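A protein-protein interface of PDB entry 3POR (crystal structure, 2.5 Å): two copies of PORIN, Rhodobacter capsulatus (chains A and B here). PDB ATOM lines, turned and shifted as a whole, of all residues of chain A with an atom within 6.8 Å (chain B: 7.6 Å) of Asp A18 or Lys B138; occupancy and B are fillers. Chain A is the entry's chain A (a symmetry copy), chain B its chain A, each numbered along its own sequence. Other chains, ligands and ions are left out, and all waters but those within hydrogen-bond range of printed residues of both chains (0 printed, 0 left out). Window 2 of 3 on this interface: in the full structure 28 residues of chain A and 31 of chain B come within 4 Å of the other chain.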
ATOM      1  N   MET A  13      -7.941  18.576  18.592  1.00  0.00           N
ATOM      2  CA  MET A  13      -6.664  17.947  18.365  1.00  0.00           C
ATOM      3  C   MET A  13      -5.775  18.192  19.541  1.00  0.00           C
ATOM      4  O   MET A  13      -5.760  19.310  20.049  1.00  0.00           O
ATOM      5  CB  MET A  13      -6.059  18.523  17.107  1.00  0.00           C
ATOM      6  CG  MET A  13      -4.837  17.765  16.593  1.00  0.00           C
ATOM      7  SD  MET A  13      -3.155  18.356  16.994  1.00  0.00           S
ATOM      8  CE  MET A  13      -3.266  19.877  16.093  1.00  0.00           C
ATOM      9  N   TYR A  14      -5.047  17.161  19.904  1.00  0.00           N
ATOM     10  CA  TYR A  14      -4.166  17.183  21.024  1.00  0.00           C
ATOM     11  C   TYR A  14      -2.748  17.098  20.495  1.00  0.00           C
ATOM     12  O   TYR A  14      -2.339  16.057  19.976  1.00  0.00           O
ATOM     13  CB  TYR A  14      -4.476  16.018  21.860  1.00  0.00           C
ATOM     14  CG  TYR A  14      -3.725  16.119  23.154  1.00  0.00           C
ATOM     15  CD1 TYR A  14      -4.152  17.039  24.085  1.00  0.00           C
ATOM     16  CD2 TYR A  14      -2.596  15.351  23.383  1.00  0.00           C
ATOM     17  CE1 TYR A  14      -3.439  17.210  25.253  1.00  0.00           C
ATOM     18  CE2 TYR A  14      -1.875  15.509  24.547  1.00  0.00           C
ATOM     19  CZ  TYR A  14      -2.305  16.447  25.467  1.00  0.00           C
ATOM     20  OH  TYR A  14      -1.558  16.712  26.594  1.00  0.00           O
ATOM     21  N   ASN A  15      -1.957  18.155  20.687  1.00  0.00           N
ATOM     22  CA  ASN A  15      -0.614  18.267  20.110  1.00  0.00           C
ATOM     23  C   ASN A  15       0.555  17.815  20.944  1.00  0.00           C
ATOM     24  O   ASN A  15       1.744  17.914  20.574  1.00  0.00           O
ATOM     25  CB  ASN A  15      -0.320  19.695  19.702  1.00  0.00           C
ATOM     26  CG  ASN A  15      -0.594  20.698  20.806  1.00  0.00           C
ATOM     27  OD1 ASN A  15      -0.611  20.399  22.013  1.00  0.00           O
ATOM     28  ND2 ASN A  15      -0.869  21.917  20.377  1.00  0.00           N
ATOM     29  N   GLY A  16       0.132  17.241  22.049  1.00  0.00           N
ATOM     30  CA  GLY A  16       1.082  16.732  22.998  1.00  0.00           C
ATOM     31  C   GLY A  16       0.826  17.320  24.377  1.00  0.00           C
ATOM     32  O   GLY A  16       1.006  16.652  25.403  1.00  0.00           O
ATOM     33  N   ASP A  17       0.271  18.542  24.401  1.00  0.00           N
ATOM     34  CA  ASP A  17       0.132  19.322  25.635  1.00  0.00           C
ATOM     35  C   ASP A  17      -1.262  19.900  25.854  1.00  0.00           C
ATOM     36  O   ASP A  17      -1.788  19.912  26.975  1.00  0.00           O
ATOM     37  CB  ASP A  17       1.172  20.495  25.620  1.00  0.00           C
ATOM     38  CG  ASP A  17       2.311  20.499  24.547  1.00  0.00           C
ATOM     39  OD1 ASP A  17       3.089  19.521  24.422  1.00  0.00           O
ATOM     40  OD2 ASP A  17       2.426  21.510  23.829  1.00  0.00           O
ATOM     41  N   ASP A  18      -1.812  20.430  24.740  1.00  0.00           N
ATOM     42  CA  ASP A  18      -3.137  21.022  24.702  1.00  0.00           C
ATOM     43  C   ASP A  18      -3.992  20.547  23.595  1.00  0.00           C
ATOM     44  O   ASP A  18      -3.493  20.133  22.543  1.00  0.00           O
ATOM     45  CB  ASP A  18      -3.119  22.478  24.500  1.00  0.00           C
ATOM     46  CG  ASP A  18      -2.445  23.173  25.645  1.00  0.00           C
ATOM     47  OD1 ASP A  18      -2.522  22.687  26.785  1.00  0.00           O
ATOM     48  OD2 ASP A  18      -1.831  24.210  25.389  1.00  0.00           O
ATOM     49  N   TRP A  19      -5.281  20.610  23.912  1.00  0.00           N
ATOM     50  CA  TRP A  19      -6.318  20.374  22.908  1.00  0.00           C
ATOM     51  C   TRP A  19      -6.593  21.644  22.097  1.00  0.00           C
ATOM     52  O   TRP A  19      -6.513  22.734  22.659  1.00  0.00           O
ATOM     53  CB  TRP A  19      -7.612  19.920  23.562  1.00  0.00           C
ATOM     54  CG  TRP A  19      -7.507  18.446  23.877  1.00  0.00           C
ATOM     55  CD1 TRP A  19      -7.181  18.079  25.142  1.00  0.00           C
ATOM     56  CD2 TRP A  19      -7.741  17.346  23.063  1.00  0.00           C
ATOM     57  NE1 TRP A  19      -7.215  16.761  25.150  1.00  0.00           N
ATOM     58  CE2 TRP A  19      -7.546  16.295  23.948  1.00  0.00           C
ATOM     59  CE3 TRP A  19      -8.080  17.020  21.769  1.00  0.00           C
ATOM     60  CZ2 TRP A  19      -7.681  14.972  23.617  1.00  0.00           C
ATOM     61  CZ3 TRP A  19      -8.216  15.682  21.425  1.00  0.00           C
ATOM     62  CH2 TRP A  19      -8.022  14.664  22.333  1.00  0.00           C
ATOM     63  N   ASN A  20      -6.881  21.639  20.796  1.00  0.00           N
ATOM     64  CA  ASN A  20      -7.224  22.864  20.097  1.00  0.00           C
ATOM     65  C   ASN A  20      -8.276  22.433  19.142  1.00  0.00           C
ATOM     66  O   ASN A  20      -8.329  21.268  18.743  1.00  0.00           O
ATOM     67  CB  ASN A  20      -6.165  23.389  19.227  1.00  0.00           C
ATOM     68  CG  ASN A  20      -4.837  23.518  19.933  1.00  0.00           C
ATOM     69  OD1 ASN A  20      -4.512  24.470  20.675  1.00  0.00           O
ATOM     70  ND2 ASN A  20      -4.049  22.473  19.671  1.00  0.00           N
ATOM     71  N   GLU B 114      -7.961  36.574  15.747  1.00  0.00           N
ATOM     72  CA  GLU B 114      -6.688  35.880  15.917  1.00  0.00           C
ATOM     73  C   GLU B 114      -6.899  34.457  16.409  1.00  0.00           C
ATOM     74  O   GLU B 114      -6.115  33.600  16.035  1.00  0.00           O
ATOM     75  CB  GLU B 114      -5.778  36.687  16.913  1.00  0.00           C
ATOM     76  CG  GLU B 114      -6.364  37.426  18.195  1.00  0.00           C
ATOM     77  CD  GLU B 114      -6.251  36.823  19.629  1.00  0.00           C
ATOM     78  OE1 GLU B 114      -5.488  35.864  19.870  1.00  0.00           O
ATOM     79  OE2 GLU B 114      -6.945  37.344  20.523  1.00  0.00           O
ATOM     80  N   ASP B 115      -7.984  34.244  17.168  1.00  0.00           N
ATOM     81  CA  ASP B 115      -8.365  33.027  17.845  1.00  0.00           C
ATOM     82  C   ASP B 115      -8.875  31.893  16.991  1.00  0.00           C
ATOM     83  O   ASP B 115      -8.824  30.728  17.413  1.00  0.00           O
ATOM     84  CB  ASP B 115      -9.442  33.327  18.875  1.00  0.00           C
ATOM     85  CG  ASP B 115      -9.001  33.819  20.257  1.00  0.00           C
ATOM     86  OD1 ASP B 115      -8.252  33.088  20.933  1.00  0.00           O
ATOM     87  OD2 ASP B 115      -9.450  34.899  20.675  1.00  0.00           O
ATOM     88  N   ASN B 116      -9.396  32.314  15.836  1.00  0.00           N
ATOM     89  CA  ASN B 116     -10.041  31.465  14.850  1.00  0.00           C
ATOM     90  C   ASN B 116      -9.320  30.165  14.460  1.00  0.00           C
ATOM     91  O   ASN B 116      -8.150  30.280  14.091  1.00  0.00           O
ATOM     92  CB  ASN B 116     -10.283  32.228  13.568  1.00  0.00           C
ATOM     93  CG  ASN B 116     -11.403  33.234  13.570  1.00  0.00           C
ATOM     94  OD1 ASN B 116     -12.061  33.608  14.557  1.00  0.00           O
ATOM     95  ND2 ASN B 116     -11.632  33.706  12.362  1.00  0.00           N
ATOM     96  N   PRO B 117      -9.861  28.911  14.353  1.00  0.00           N
ATOM     97  CA  PRO B 117     -11.273  28.623  14.226  1.00  0.00           C
ATOM     98  C   PRO B 117     -11.870  28.810  15.609  1.00  0.00           C
ATOM     99  O   PRO B 117     -11.359  28.303  16.619  1.00  0.00           O
ATOM    100  CB  PRO B 117     -11.322  27.194  13.740  1.00  0.00           C
ATOM    101  CG  PRO B 117      -9.891  26.780  13.480  1.00  0.00           C
ATOM    102  CD  PRO B 117      -9.119  27.643  14.430  1.00  0.00           C
ATOM    103  N   VAL B 118     -12.904  29.643  15.630  1.00  0.00           N
ATOM    104  CA  VAL B 118     -13.740  29.736  16.809  1.00  0.00           C
ATOM    105  C   VAL B 118     -14.958  28.800  16.598  1.00  0.00           C
ATOM    106  O   VAL B 118     -15.144  28.299  15.482  1.00  0.00           O
ATOM    107  CB  VAL B 118     -14.079  31.204  16.979  1.00  0.00           C
ATOM    108  CG1 VAL B 118     -12.726  31.816  17.307  1.00  0.00           C
ATOM    109  CG2 VAL B 118     -14.664  31.906  15.788  1.00  0.00           C
ATOM    110  N   SER B 135     -13.532  30.529  21.714  1.00  0.00           N
ATOM    111  CA  SER B 135     -12.300  30.057  21.144  1.00  0.00           C
ATOM    112  C   SER B 135     -11.894  28.904  22.010  1.00  0.00           C
ATOM    113  O   SER B 135     -12.523  28.552  22.996  1.00  0.00           O
ATOM    114  CB  SER B 135     -11.218  31.092  21.225  1.00  0.00           C
ATOM    115  OG  SER B 135     -11.135  31.749  22.484  1.00  0.00           O
ATOM    116  N   ASP B 136     -10.819  28.270  21.604  1.00  0.00           N
ATOM    117  CA  ASP B 136     -10.156  27.229  22.393  1.00  0.00           C
ATOM    118  C   ASP B 136      -9.230  27.720  23.528  1.00  0.00           C
ATOM    119  O   ASP B 136      -8.775  26.890  24.327  1.00  0.00           O
ATOM    120  CB  ASP B 136      -9.327  26.322  21.455  1.00  0.00           C
ATOM    121  CG  ASP B 136      -8.531  26.916  20.275  1.00  0.00           C
ATOM    122  OD1 ASP B 136      -8.552  28.135  20.030  1.00  0.00           O
ATOM    123  OD2 ASP B 136      -7.905  26.120  19.574  1.00  0.00           O
ATOM    124  N   GLY B 137      -8.876  29.035  23.597  1.00  0.00           N
ATOM    125  CA  GLY B 137      -7.967  29.603  24.634  1.00  0.00           C
ATOM    126  C   GLY B 137      -6.441  29.494  24.365  1.00  0.00           C
ATOM    127  O   GLY B 137      -5.564  29.769  25.214  1.00  0.00           O
ATOM    128  N   LYS B 138      -6.224  29.101  23.090  1.00  0.00           N
ATOM    129  CA  LYS B 138      -4.961  28.880  22.403  1.00  0.00           C
ATOM    130  C   LYS B 138      -5.131  29.612  21.054  1.00  0.00           C
ATOM    131  O   LYS B 138      -6.270  30.046  20.730  1.00  0.00           O
ATOM    132  CB  LYS B 138      -4.724  27.357  22.223  1.00  0.00           C
ATOM    133  CG  LYS B 138      -4.656  26.609  23.556  1.00  0.00           C
ATOM    134  CD  LYS B 138      -3.513  27.211  24.350  1.00  0.00           C
ATOM    135  CE  LYS B 138      -3.470  27.028  25.860  1.00  0.00           C
ATOM    136  NZ  LYS B 138      -2.094  27.245  26.307  1.00  0.00           N
ATOM    137  N   VAL B 139      -4.036  29.821  20.272  1.00  0.00           N
ATOM    138  CA  VAL B 139      -4.120  30.495  18.961  1.00  0.00           C
ATOM    139  C   VAL B 139      -4.330  29.442  17.836  1.00  0.00           C
ATOM    140  O   VAL B 139      -3.445  29.003  17.076  1.00  0.00           O
ATOM    141  CB  VAL B 139      -2.799  31.405  18.840  1.00  0.00           C
ATOM    142  CG1 VAL B 139      -1.517  30.698  18.388  1.00  0.00           C
ATOM    143  CG2 VAL B 139      -3.177  32.535  17.884  1.00  0.00           C
ATOM    144  N   GLY B 140      -5.590  28.989  17.735  1.00  0.00           N
ATOM    145  CA  GLY B 140      -5.930  27.869  16.868  1.00  0.00           C
ATOM    146  C   GLY B 140      -5.179  26.648  17.413  1.00  0.00           C
ATOM    147  O   GLY B 140      -5.138  26.447  18.633  1.00  0.00           O
ATOM    148  N   GLU B 141      -4.497  25.869  16.562  1.00  0.00           N
ATOM    149  CA  GLU B 141      -3.744  24.693  17.005  1.00  0.00           C
ATOM    150  C   GLU B 141      -2.362  24.964  17.629  1.00  0.00           C
ATOM    151  O   GLU B 141      -1.698  24.022  18.110  1.00  0.00           O
ATOM    152  CB  GLU B 141      -3.558  23.694  15.840  1.00  0.00           C
ATOM    153  CG  GLU B 141      -4.828  23.154  15.180  1.00  0.00           C
ATOM    154  CD  GLU B 141      -5.281  23.912  13.928  1.00  0.00           C
ATOM    155  OE1 GLU B 141      -4.849  23.542  12.829  1.00  0.00           O
ATOM    156  OE2 GLU B 141      -6.078  24.853  14.050  1.00  0.00           O
ATOM    157  N   THR B 142      -1.849  26.206  17.611  1.00  0.00           N
ATOM    158  CA  THR B 142      -0.592  26.494  18.285  1.00  0.00           C
ATOM    159  C   THR B 142      -1.065  26.934  19.667  1.00  0.00           C
ATOM    160  O   THR B 142      -1.724  27.962  19.881  1.00  0.00           O
ATOM    161  CB  THR B 142       0.203  27.627  17.574  1.00  0.00           C
ATOM    162  OG1 THR B 142       0.233  27.302  16.187  1.00  0.00           O
ATOM    163  CG2 THR B 142       1.641  27.756  18.091  1.00  0.00           C
ATOM    164  N   SER B 143      -0.810  26.034  20.604  1.00  0.00           N
ATOM    165  CA  SER B 143      -1.171  26.242  21.984  1.00  0.00           C
ATOM    166  C   SER B 143      -0.463  27.407  22.681  1.00  0.00           C
ATOM    167  O   SER B 143       0.565  27.338  23.357  1.00  0.00           O
ATOM    168  CB  SER B 143      -0.931  24.911  22.619  1.00  0.00           C
ATOM    169  OG  SER B 143      -1.832  23.976  22.038  1.00  0.00           O
ATOM    170  N   GLU B 144      -1.109  28.530  22.401  1.00  0.00           N
ATOM    171  CA  GLU B 144      -0.720  29.849  22.858  1.00  0.00           C
ATOM    172  C   GLU B 144      -1.672  30.212  23.997  1.00  0.00           C
ATOM    173  O   GLU B 144      -2.880  30.239  23.748  1.00  0.00           O
ATOM    174  CB  GLU B 144      -0.858  30.845  21.676  1.00  0.00           C
ATOM    175  CG  GLU B 144      -0.591  32.350  21.905  1.00  0.00           C
ATOM    176  CD  GLU B 144      -0.819  33.316  20.728  1.00  0.00           C
ATOM    177  OE1 GLU B 144       0.013  33.368  19.811  1.00  0.00           O
ATOM    178  OE2 GLU B 144      -1.830  34.030  20.728  1.00  0.00           O
ATOM    179  N   ASP B 145      -1.194  30.463  25.230  1.00  0.00           N
ATOM    180  CA  ASP B 145      -2.044  30.914  26.347  1.00  0.00           C
ATOM    181  C   ASP B 145      -2.592  32.320  25.995  1.00  0.00           C
ATOM    182  O   ASP B 145      -1.843  33.328  25.964  1.00  0.00           O
ATOM    183  CB  ASP B 145      -1.182  30.935  27.669  1.00  0.00           C
ATOM    184  CG  ASP B 145      -1.922  31.128  29.018  1.00  0.00           C
ATOM    185  OD1 ASP B 145      -2.652  30.212  29.434  1.00  0.00           O
ATOM    186  OD2 ASP B 145      -1.754  32.183  29.661  1.00  0.00           O
ATOM    187  N   ASP B 146      -3.893  32.383  25.663  1.00  0.00           N
ATOM    188  CA  ASP B 146      -4.442  33.655  25.255  1.00  0.00           C
ATOM    189  C   ASP B 146      -5.892  33.823  25.699  1.00  0.00           C
ATOM    190  O   ASP B 146      -6.392  33.299  26.724  1.00  0.00           O
ATOM    191  CB  ASP B 146      -4.229  33.796  23.653  1.00  0.00           C
ATOM    192  CG  ASP B 146      -4.946  32.936  22.577  1.00  0.00           C
ATOM    193  OD1 ASP B 146      -5.928  32.250  22.859  1.00  0.00           O
ATOM    194  OD2 ASP B 146      -4.527  32.981  21.417  1.00  0.00           O
ATOM    195  N   ALA B 147      -6.410  34.787  24.910  1.00  0.00           N
ATOM    196  CA  ALA B 147      -7.807  35.157  24.816  1.00  0.00           C
ATOM    197  C   ALA B 147      -8.706  33.939  24.727  1.00  0.00           C
ATOM    198  O   ALA B 147      -8.747  33.088  23.811  1.00  0.00           O
ATOM    199  CB  ALA B 147      -8.086  36.021  23.565  1.00  0.00           C
ATOM    200  N   GLN B 148      -9.270  33.878  25.898  1.00  0.00           N
ATOM    201  CA  GLN B 148     -10.344  33.012  26.038  1.00  0.00           C
ATOM    202  C   GLN B 148     -11.459  34.010  25.836  1.00  0.00           C
ATOM    203  O   GLN B 148     -11.530  35.015  26.531  1.00  0.00           O
ATOM    204  CB  GLN B 148     -10.226  32.392  27.400  1.00  0.00           C
ATOM    205  CG  GLN B 148     -11.451  31.513  27.642  1.00  0.00           C
ATOM    206  CD  GLN B 148     -11.988  30.658  26.464  1.00  0.00           C
ATOM    207  OE1 GLN B 148     -11.327  30.431  25.443  1.00  0.00           O
ATOM    208  NE2 GLN B 148     -13.223  30.153  26.492  1.00  0.00           N
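Among the printed residues, pairs that only touch across the chains: Met A13 with Glu B141 (3.7 Å), Asn A20 with Asp B136 (3.3 Å) and Asn A20 with Lys B138 (3.3 Å).
Of the printed residues of chain B, Met A13 touches Glu B141.
Printed residues of chain B within 4 Å of Asn A15: Glu B141 and Ser B143.
Asp A18 touches two residues of chain B.
Of the printed residues of chain B, Asn A20 touches Asp B136, Lys B138, Gly B140, Glu B141 and Ser B143.
No residue of chain A comes within 4 Å of Gly B137.
Lys B138 touches two residues of chain A.
Printed residues of chain A within 4 Å of Gly B140: Asn A20 (2.9 Å).
Of the printed residues of chain A, Ser B143 touches Asn A15, Asp A18 and Asn A20.
The nearest residue of chain B that does not touch Asp A18 is Glu B144 (5.3 Å).
The nearest residue of chain A that does not touch Lys B138 is Trp A19 (4.4 Å).
The nearest printed residue of chain A that does not touch Gly B140 is Trp A19 (5.6 Å).
Of the 8 printed residues of chain A, 4 touch a printed residue of chain B.
Hydrophobic or aromatic side chains of chain A that line the printed part of chain B: Met A13.
Among the printed residues, 10 pairs touch across the chains.
No position is printed for both chains.
Of the 10 pairs that touch across the chains among the printed residues, none has its exchanged pair printed and touching as well.
The side-chain hydroxyl (OG) of Ser B143 is in hydrogen-bond range of the side-chain amide oxygen (OD1) of Asn A20 (3.0 Å).
The side-chain hydroxyl (OG) of Ser B143 sits at hydrogen-bond distance from the side-chain amide nitrogen (ND2) of Asn A15 (2.8 Å).
OD2 of Asp A18 is in salt-bridge range of NZ of Lys B138 (3.2 Å).
The backbone carbonyl oxygen (O) of Glu B141 lies within hydrogen-bond range of the side-chain amide nitrogen (ND2) of Asn A20 (3.2 Å).
The backbone carbonyl oxygen (O) of Gly B140 lies close to the side-chain amide oxygen (OD1) of Asn A20 (2.9 Å).
The backbone carbonyl oxygen (O) of Glu B141 lies within hydrogen-bond range of the side-chain amide nitrogen (ND2) of Asn A15 (3.2 Å).
The side-chain hydroxyl of Ser B143 lies close to the side-chain carboxylate of Asp A18 (3.4 Å).
OD1 of Asn A15 sits close to O of Asp A18, at 2.9 Å.
The backbone carbonyl oxygen of Met A13 lies within hydrogen-bond range of the backbone NH of Asn A20, 2.7 Å away.
The side-chain amide nitrogen (ND2) of Asn A15 sits close to the side-chain amide nitrogen (ND2) of Asn A20 (3.3 Å).
The backbone NH of Lys B138 lies within hydrogen-bond range of the side-chain carboxylate of Asp B146, at 3.2 Å.
The side-chain amide oxygen of Asn A15 sits at hydrogen-bond distance from the backbone NH of Asp A17 (3.2 Å).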
